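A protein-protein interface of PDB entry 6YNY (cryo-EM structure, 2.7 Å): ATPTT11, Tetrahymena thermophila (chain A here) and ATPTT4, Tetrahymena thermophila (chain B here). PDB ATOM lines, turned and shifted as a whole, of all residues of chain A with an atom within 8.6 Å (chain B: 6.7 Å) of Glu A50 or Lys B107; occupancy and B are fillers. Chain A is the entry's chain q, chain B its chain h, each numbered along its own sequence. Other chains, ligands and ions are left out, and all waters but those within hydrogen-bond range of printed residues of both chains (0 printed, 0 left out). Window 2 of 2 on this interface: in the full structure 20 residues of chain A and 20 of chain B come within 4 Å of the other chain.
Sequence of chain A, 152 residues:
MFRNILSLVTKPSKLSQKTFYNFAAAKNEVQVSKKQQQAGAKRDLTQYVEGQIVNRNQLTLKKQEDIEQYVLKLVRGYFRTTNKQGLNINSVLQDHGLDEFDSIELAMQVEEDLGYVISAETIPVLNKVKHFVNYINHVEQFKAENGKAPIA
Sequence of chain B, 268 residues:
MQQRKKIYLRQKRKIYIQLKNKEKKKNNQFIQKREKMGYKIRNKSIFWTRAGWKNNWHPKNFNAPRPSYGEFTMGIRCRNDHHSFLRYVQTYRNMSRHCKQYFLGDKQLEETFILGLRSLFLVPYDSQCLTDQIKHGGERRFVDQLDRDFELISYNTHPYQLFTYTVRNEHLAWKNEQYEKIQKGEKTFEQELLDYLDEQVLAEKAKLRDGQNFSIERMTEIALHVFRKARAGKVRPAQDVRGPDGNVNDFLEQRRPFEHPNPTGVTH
NZ of Lys B107 lies within salt-bridge range of OE1 of Glu B110, 3.9 Å away.
Printed residues of chain B that touch a printed residue of chain A: Leu B104, Gly B105, Lys B107 and Glu B111. Of the 13 printed residues of chain A, 4 touch a printed residue of chain B. Hydrophobic or aromatic side chains of chain A that line the printed part of chain B: Tyr A48 and Phe A79.
N of Glu A50 is in hydrogen-bond range of O of Gly B105 (3.1 Å). The backbone NH (N) of Gly A51 sits at hydrogen-bond distance from the backbone carbonyl oxygen (O) of Leu B104, 2.9 Å away.
Of chain A, only Glu A50 comes within 4 Å of Lys B107. Of the printed residues of chain B, Tyr A48 touches Leu B104 (3.4 Å) and Gly B105 (3.3 Å). Printed residues of chain A within 4 Å of Glu B111: Phe A79 (3.7 Å). Of the printed residues of chain B, Gly A51 touches Leu B104. Of the printed residues of chain A, Leu B104 touches Tyr A48 (3.4 Å), Glu A50 (3.7 Å) and Gly A51 (2.9 Å). Tyr A78 touches none of the printed residues of chain B. The nearest residue of chain B that does not touch Glu A50 is Asp B106 (4.2 Å). The nearest printed residue of chain A that does not touch Glu B111 is Gly A77 (5.7 Å).
Leu B104 touches Tyr A48. Tyr A48 touches Gly B105. Glu A50 touches Leu B104. OE2 of Glu A50 touches N of Lys B107 (3.6 Å). Phe A79 touches Glu B111.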
ATOM      1  N   GLN A  47     -29.760   8.408 -21.012  1.00  0.00           N
ATOM      2  CA  GLN A  47     -29.239   9.596 -21.666  1.00  0.00           C
ATOM      3  C   GLN A  47     -29.785   9.670 -23.082  1.00  0.00           C
ATOM      4  O   GLN A  47     -30.162   8.661 -23.680  1.00  0.00           O
ATOM      5  CB  GLN A  47     -27.707   9.595 -21.710  1.00  0.00           C
ATOM      6  CG  GLN A  47     -27.040   9.694 -20.357  1.00  0.00           C
ATOM      7  CD  GLN A  47     -25.532   9.761 -20.464  1.00  0.00           C
ATOM      8  OE1 GLN A  47     -24.967   9.609 -21.546  1.00  0.00           O
ATOM      9  NE2 GLN A  47     -24.872   9.992 -19.340  1.00  0.00           N
ATOM     10  N   TYR A  48     -29.825  10.887 -23.613  1.00  0.00           N
ATOM     11  CA  TYR A  48     -30.216  11.097 -24.996  1.00  0.00           C
ATOM     12  C   TYR A  48     -29.054  10.780 -25.922  1.00  0.00           C
ATOM     13  O   TYR A  48     -27.905  11.138 -25.649  1.00  0.00           O
ATOM     14  CB  TYR A  48     -30.672  12.535 -25.222  1.00  0.00           C
ATOM     15  CG  TYR A  48     -32.106  12.810 -24.857  1.00  0.00           C
ATOM     16  CD1 TYR A  48     -32.430  13.434 -23.667  1.00  0.00           C
ATOM     17  CD2 TYR A  48     -33.136  12.456 -25.710  1.00  0.00           C
ATOM     18  CE1 TYR A  48     -33.740  13.692 -23.335  1.00  0.00           C
ATOM     19  CE2 TYR A  48     -34.448  12.708 -25.386  1.00  0.00           C
ATOM     20  CZ  TYR A  48     -34.745  13.327 -24.195  1.00  0.00           C
ATOM     21  OH  TYR A  48     -36.052  13.582 -23.867  1.00  0.00           O
ATOM     22  N   VAL A  49     -29.358  10.100 -27.022  1.00  0.00           N
ATOM     23  CA  VAL A  49     -28.376   9.779 -28.049  1.00  0.00           C
ATOM     24  C   VAL A  49     -29.029  10.062 -29.393  1.00  0.00           C
ATOM     25  O   VAL A  49     -29.887   9.293 -29.843  1.00  0.00           O
ATOM     26  CB  VAL A  49     -27.894   8.327 -27.970  1.00  0.00           C
ATOM     27  CG1 VAL A  49     -26.865   8.055 -29.042  1.00  0.00           C
ATOM     28  CG2 VAL A  49     -27.316   8.051 -26.602  1.00  0.00           C
ATOM     29  N   GLU A  50     -28.631  11.160 -30.032  1.00  0.00           N
ATOM     30  CA  GLU A  50     -29.194  11.566 -31.316  1.00  0.00           C
ATOM     31  C   GLU A  50     -30.706  11.740 -31.221  1.00  0.00           C
ATOM     32  O   GLU A  50     -31.450  11.397 -32.141  1.00  0.00           O
ATOM     33  CB  GLU A  50     -28.828  10.567 -32.412  1.00  0.00           C
ATOM     34  CG  GLU A  50     -27.337  10.461 -32.665  1.00  0.00           C
ATOM     35  CD  GLU A  50     -26.747  11.743 -33.218  1.00  0.00           C
ATOM     36  OE1 GLU A  50     -27.525  12.646 -33.592  1.00  0.00           O
ATOM     37  OE2 GLU A  50     -25.504  11.849 -33.281  1.00  0.00           O
ATOM     38  N   GLY A  51     -31.163  12.281 -30.095  1.00  0.00           N
ATOM     39  CA  GLY A  51     -32.563  12.564 -29.883  1.00  0.00           C
ATOM     40  C   GLY A  51     -33.365  11.436 -29.281  1.00  0.00           C
ATOM     41  O   GLY A  51     -34.552  11.630 -28.991  1.00  0.00           O
ATOM     42  N   GLN A  52     -32.765  10.268 -29.082  1.00  0.00           N
ATOM     43  CA  GLN A  52     -33.453   9.110 -28.532  1.00  0.00           C
ATOM     44  C   GLN A  52     -32.890   8.770 -27.161  1.00  0.00           C
ATOM     45  O   GLN A  52     -31.672   8.782 -26.957  1.00  0.00           O
ATOM     46  CB  GLN A  52     -33.320   7.908 -29.464  1.00  0.00           C
ATOM     47  CG  GLN A  52     -33.875   8.150 -30.851  1.00  0.00           C
ATOM     48  CD  GLN A  52     -35.361   8.432 -30.837  1.00  0.00           C
ATOM     49  OE1 GLN A  52     -36.082   7.971 -29.953  1.00  0.00           O
ATOM     50  NE2 GLN A  52     -35.826   9.196 -31.815  1.00  0.00           N
ATOM     51  N   ILE A  53     -33.783   8.466 -26.226  1.00  0.00           N
ATOM     52  CA  ILE A  53     -33.387   8.095 -24.874  1.00  0.00           C
ATOM     53  C   ILE A  53     -32.891   6.656 -24.890  1.00  0.00           C
ATOM     54  O   ILE A  53     -33.608   5.746 -25.316  1.00  0.00           O
ATOM     55  CB  ILE A  53     -34.550   8.273 -23.889  1.00  0.00           C
ATOM     56  CG1 ILE A  53     -34.939   9.750 -23.809  1.00  0.00           C
ATOM     57  CG2 ILE A  53     -34.169   7.745 -22.519  1.00  0.00           C
ATOM     58  CD1 ILE A  53     -36.159  10.026 -22.976  1.00  0.00           C
ATOM     59  N   VAL A  54     -31.664   6.452 -24.423  1.00  0.00           N
ATOM     60  CA  VAL A  54     -31.032   5.142 -24.399  1.00  0.00           C
ATOM     61  C   VAL A  54     -30.518   4.879 -22.993  1.00  0.00           C
ATOM     62  O   VAL A  54     -30.008   5.787 -22.328  1.00  0.00           O
ATOM     63  CB  VAL A  54     -29.880   5.049 -25.420  1.00  0.00           C
ATOM     64  CG1 VAL A  54     -29.279   3.656 -25.416  1.00  0.00           C
ATOM     65  CG2 VAL A  54     -30.370   5.420 -26.800  1.00  0.00           C
ATOM     66  N   GLY A  77     -11.749   7.573 -29.852  1.00  0.00           N
ATOM     67  CA  GLY A  77     -13.084   8.084 -30.085  1.00  0.00           C
ATOM     68  C   GLY A  77     -13.192   9.590 -30.049  1.00  0.00           C
ATOM     69  O   GLY A  77     -14.183  10.140 -30.539  1.00  0.00           O
ATOM     70  N   TYR A  78     -12.201  10.267 -29.480  1.00  0.00           N
ATOM     71  CA  TYR A  78     -12.237  11.716 -29.367  1.00  0.00           C
ATOM     72  C   TYR A  78     -11.925  12.351 -30.715  1.00  0.00           C
ATOM     73  O   TYR A  78     -10.939  11.998 -31.368  1.00  0.00           O
ATOM     74  CB  TYR A  78     -11.243  12.178 -28.304  1.00  0.00           C
ATOM     75  CG  TYR A  78     -11.509  13.556 -27.753  1.00  0.00           C
ATOM     76  CD1 TYR A  78     -12.742  13.882 -27.217  1.00  0.00           C
ATOM     77  CD2 TYR A  78     -10.520  14.521 -27.748  1.00  0.00           C
ATOM     78  CE1 TYR A  78     -12.986  15.134 -26.711  1.00  0.00           C
ATOM     79  CE2 TYR A  78     -10.756  15.776 -27.244  1.00  0.00           C
ATOM     80  CZ  TYR A  78     -11.989  16.078 -26.725  1.00  0.00           C
ATOM     81  OH  TYR A  78     -12.219  17.333 -26.221  1.00  0.00           O
ATOM     82  N   PHE A  79     -12.776  13.290 -31.130  1.00  0.00           N
ATOM     83  CA  PHE A  79     -12.685  13.885 -32.456  1.00  0.00           C
ATOM     84  C   PHE A  79     -11.445  14.747 -32.643  1.00  0.00           C
ATOM     85  O   PHE A  79     -11.148  15.130 -33.779  1.00  0.00           O
ATOM     86  CB  PHE A  79     -13.937  14.715 -32.731  1.00  0.00           C
ATOM     87  CG  PHE A  79     -13.988  16.011 -31.977  1.00  0.00           C
ATOM     88  CD1 PHE A  79     -13.810  17.213 -32.631  1.00  0.00           C
ATOM     89  CD2 PHE A  79     -14.215  16.029 -30.617  1.00  0.00           C
ATOM     90  CE1 PHE A  79     -13.857  18.401 -31.946  1.00  0.00           C
ATOM     91  CE2 PHE A  79     -14.262  17.217 -29.927  1.00  0.00           C
ATOM     92  CZ  PHE A  79     -14.083  18.402 -30.592  1.00  0.00           C
ATOM     93  N   GLU A 105     -12.159  16.384 -20.983  1.00  0.00           N
ATOM     94  CA  GLU A 105     -13.233  15.728 -21.719  1.00  0.00           C
ATOM     95  C   GLU A 105     -13.067  14.216 -21.720  1.00  0.00           C
ATOM     96  O   GLU A 105     -14.059  13.481 -21.710  1.00  0.00           O
ATOM     97  CB  GLU A 105     -13.278  16.251 -23.151  1.00  0.00           C
ATOM     98  CG  GLU A 105     -13.746  17.682 -23.278  1.00  0.00           C
ATOM     99  CD  GLU A 105     -15.223  17.842 -22.992  1.00  0.00           C
ATOM    100  OE1 GLU A 105     -15.899  16.821 -22.749  1.00  0.00           O
ATOM    101  OE2 GLU A 105     -15.710  18.991 -23.014  1.00  0.00           O
ATOM    102  N   GLN A 109     -15.453  11.438 -19.767  1.00  0.00           N
ATOM    103  CA  GLN A 109     -16.000  10.261 -20.422  1.00  0.00           C
ATOM    104  C   GLN A 109     -15.720   8.995 -19.626  1.00  0.00           C
ATOM    105  O   GLN A 109     -16.496   8.038 -19.695  1.00  0.00           O
ATOM    106  CB  GLN A 109     -15.422  10.137 -21.828  1.00  0.00           C
ATOM    107  CG  GLN A 109     -16.122   9.120 -22.690  1.00  0.00           C
ATOM    108  CD  GLN A 109     -17.551   9.503 -22.992  1.00  0.00           C
ATOM    109  OE1 GLN A 109     -17.907  10.680 -22.979  1.00  0.00           O
ATOM    110  NE2 GLN A 109     -18.382   8.509 -23.261  1.00  0.00           N
ATOM    111  N   PHE B 103     -28.408  19.304 -25.154  1.00  0.00           N
ATOM    112  CA  PHE B 103     -28.041  19.023 -26.534  1.00  0.00           C
ATOM    113  C   PHE B 103     -28.747  17.801 -27.098  1.00  0.00           C
ATOM    114  O   PHE B 103     -28.692  17.581 -28.313  1.00  0.00           O
ATOM    115  CB  PHE B 103     -26.524  18.833 -26.650  1.00  0.00           C
ATOM    116  CG  PHE B 103     -25.726  20.085 -26.410  1.00  0.00           C
ATOM    117  CD1 PHE B 103     -26.331  21.327 -26.373  1.00  0.00           C
ATOM    118  CD2 PHE B 103     -24.361  20.013 -26.228  1.00  0.00           C
ATOM    119  CE1 PHE B 103     -25.591  22.462 -26.156  1.00  0.00           C
ATOM    120  CE2 PHE B 103     -23.622  21.148 -26.008  1.00  0.00           C
ATOM    121  CZ  PHE B 103     -24.238  22.374 -25.973  1.00  0.00           C
ATOM    122  N   LEU B 104     -29.406  17.006 -26.257  1.00  0.00           N
ATOM    123  CA  LEU B 104     -30.223  15.884 -26.709  1.00  0.00           C
ATOM    124  C   LEU B 104     -29.396  14.836 -27.442  1.00  0.00           C
ATOM    125  O   LEU B 104     -29.886  14.173 -28.357  1.00  0.00           O
ATOM    126  CB  LEU B 104     -31.368  16.371 -27.598  1.00  0.00           C
ATOM    127  CG  LEU B 104     -32.235  17.470 -26.987  1.00  0.00           C
ATOM    128  CD1 LEU B 104     -33.233  17.996 -27.994  1.00  0.00           C
ATOM    129  CD2 LEU B 104     -32.944  16.960 -25.758  1.00  0.00           C
ATOM    130  N   GLY B 105     -28.141  14.669 -27.037  1.00  0.00           N
ATOM    131  CA  GLY B 105     -27.283  13.677 -27.645  1.00  0.00           C
ATOM    132  C   GLY B 105     -26.788  14.010 -29.031  1.00  0.00           C
ATOM    133  O   GLY B 105     -26.227  13.136 -29.696  1.00  0.00           O
ATOM    134  N   ASP B 106     -26.974  15.242 -29.490  1.00  0.00           N
ATOM    135  CA  ASP B 106     -26.497  15.656 -30.805  1.00  0.00           C
ATOM    136  C   ASP B 106     -24.976  15.696 -30.774  1.00  0.00           C
ATOM    137  O   ASP B 106     -24.376  16.638 -30.254  1.00  0.00           O
ATOM    138  CB  ASP B 106     -27.078  17.015 -31.171  1.00  0.00           C
ATOM    139  CG  ASP B 106     -26.877  17.364 -32.629  1.00  0.00           C
ATOM    140  OD1 ASP B 106     -25.941  16.820 -33.250  1.00  0.00           O
ATOM    141  OD2 ASP B 106     -27.655  18.186 -33.155  1.00  0.00           O
ATOM    142  N   LYS B 107     -24.345  14.671 -31.346  1.00  0.00           N
ATOM    143  CA  LYS B 107     -22.894  14.556 -31.263  1.00  0.00           C
ATOM    144  C   LYS B 107     -22.201  15.693 -32.000  1.00  0.00           C
ATOM    145  O   LYS B 107     -21.198  16.231 -31.519  1.00  0.00           O
ATOM    146  CB  LYS B 107     -22.450  13.207 -31.821  1.00  0.00           C
ATOM    147  CG  LYS B 107     -21.015  12.847 -31.510  1.00  0.00           C
ATOM    148  CD  LYS B 107     -20.827  12.578 -30.031  1.00  0.00           C
ATOM    149  CE  LYS B 107     -19.425  12.099 -29.725  1.00  0.00           C
ATOM    150  NZ  LYS B 107     -19.223  11.903 -28.268  1.00  0.00           N
ATOM    151  N   GLN B 108     -22.716  16.071 -33.170  1.00  0.00           N
ATOM    152  CA  GLN B 108     -22.105  17.156 -33.927  1.00  0.00           C
ATOM    153  C   GLN B 108     -22.186  18.476 -33.177  1.00  0.00           C
ATOM    154  O   GLN B 108     -21.337  19.354 -33.373  1.00  0.00           O
ATOM    155  CB  GLN B 108     -22.777  17.280 -35.291  1.00  0.00           C
ATOM    156  CG  GLN B 108     -22.150  18.307 -36.200  1.00  0.00           C
ATOM    157  CD  GLN B 108     -22.773  18.321 -37.576  1.00  0.00           C
ATOM    158  OE1 GLN B 108     -23.887  17.837 -37.771  1.00  0.00           O
ATOM    159  NE2 GLN B 108     -22.053  18.870 -38.542  1.00  0.00           N
ATOM    160  N   LEU B 109     -23.195  18.641 -32.323  1.00  0.00           N
ATOM    161  CA  LEU B 109     -23.310  19.865 -31.543  1.00  0.00           C
ATOM    162  C   LEU B 109     -22.393  19.835 -30.329  1.00  0.00           C
ATOM    163  O   LEU B 109     -21.826  20.865 -29.950  1.00  0.00           O
ATOM    164  CB  LEU B 109     -24.759  20.074 -31.111  1.00  0.00           C
ATOM    165  CG  LEU B 109     -25.059  21.370 -30.361  1.00  0.00           C
ATOM    166  CD1 LEU B 109     -24.771  22.581 -31.223  1.00  0.00           C
ATOM    167  CD2 LEU B 109     -26.490  21.375 -29.897  1.00  0.00           C
ATOM    168  N   GLU B 110     -22.241  18.667 -29.704  1.00  0.00           N
ATOM    169  CA  GLU B 110     -21.320  18.550 -28.580  1.00  0.00           C
ATOM    170  C   GLU B 110     -19.898  18.882 -29.005  1.00  0.00           C
ATOM    171  O   GLU B 110     -19.169  19.571 -28.284  1.00  0.00           O
ATOM    172  CB  GLU B 110     -21.386  17.141 -27.995  1.00  0.00           C
ATOM    173  CG  GLU B 110     -22.724  16.785 -27.387  1.00  0.00           C
ATOM    174  CD  GLU B 110     -22.766  15.368 -26.851  1.00  0.00           C
ATOM    175  OE1 GLU B 110     -21.768  14.636 -27.020  1.00  0.00           O
ATOM    176  OE2 GLU B 110     -23.796  14.987 -26.258  1.00  0.00           O
ATOM    177  N   GLU B 111     -19.490  18.405 -30.179  1.00  0.00           N
ATOM    178  CA  GLU B 111     -18.141  18.675 -30.659  1.00  0.00           C
ATOM    179  C   GLU B 111     -17.982  20.131 -31.067  1.00  0.00           C
ATOM    180  O   GLU B 111     -16.919  20.727 -30.863  1.00  0.00           O
ATOM    181  CB  GLU B 111     -17.818  17.749 -31.824  1.00  0.00           C
ATOM    182  CG  GLU B 111     -17.920  16.278 -31.480  1.00  0.00           C
ATOM    183  CD  GLU B 111     -17.817  15.384 -32.698  1.00  0.00           C
ATOM    184  OE1 GLU B 111     -17.820  15.914 -33.828  1.00  0.00           O
ATOM    185  OE2 GLU B 111     -17.735  14.151 -32.526  1.00  0.00           O
ATOM    186  N   THR B 112     -19.026  20.722 -31.646  1.00  0.00           N
ATOM    187  CA  THR B 112     -18.977  22.140 -31.985  1.00  0.00           C
ATOM    188  C   THR B 112     -18.920  22.997 -30.729  1.00  0.00           C
ATOM    189  O   THR B 112     -18.177  23.983 -30.674  1.00  0.00           O
ATOM    190  CB  THR B 112     -20.191  22.515 -32.830  1.00  0.00           C
ATOM    191  OG1 THR B 112     -20.208  21.731 -34.026  1.00  0.00           O
ATOM    192  CG2 THR B 112     -20.160  23.980 -33.188  1.00  0.00           C
ATOM    193  N   ARG B 168     -29.243  26.081 -33.916  1.00  0.00           N
ATOM    194  CA  ARG B 168     -29.308  24.670 -34.276  1.00  0.00           C
ATOM    195  C   ARG B 168     -30.671  24.305 -34.847  1.00  0.00           C
ATOM    196  O   ARG B 168     -30.759  23.544 -35.817  1.00  0.00           O
ATOM    197  CB  ARG B 168     -28.987  23.806 -33.059  1.00  0.00           C
ATOM    198  CG  ARG B 168     -28.783  22.344 -33.369  1.00  0.00           C
ATOM    199  CD  ARG B 168     -27.567  22.135 -34.234  1.00  0.00           C
ATOM    200  NE  ARG B 168     -27.261  20.727 -34.437  1.00  0.00           N
ATOM    201  CZ  ARG B 168     -26.321  20.287 -35.265  1.00  0.00           C
ATOM    202  NH1 ARG B 168     -25.603  21.145 -35.968  1.00  0.00           N
ATOM    203  NH2 ARG B 168     -26.102  18.990 -35.394  1.00  0.00           N
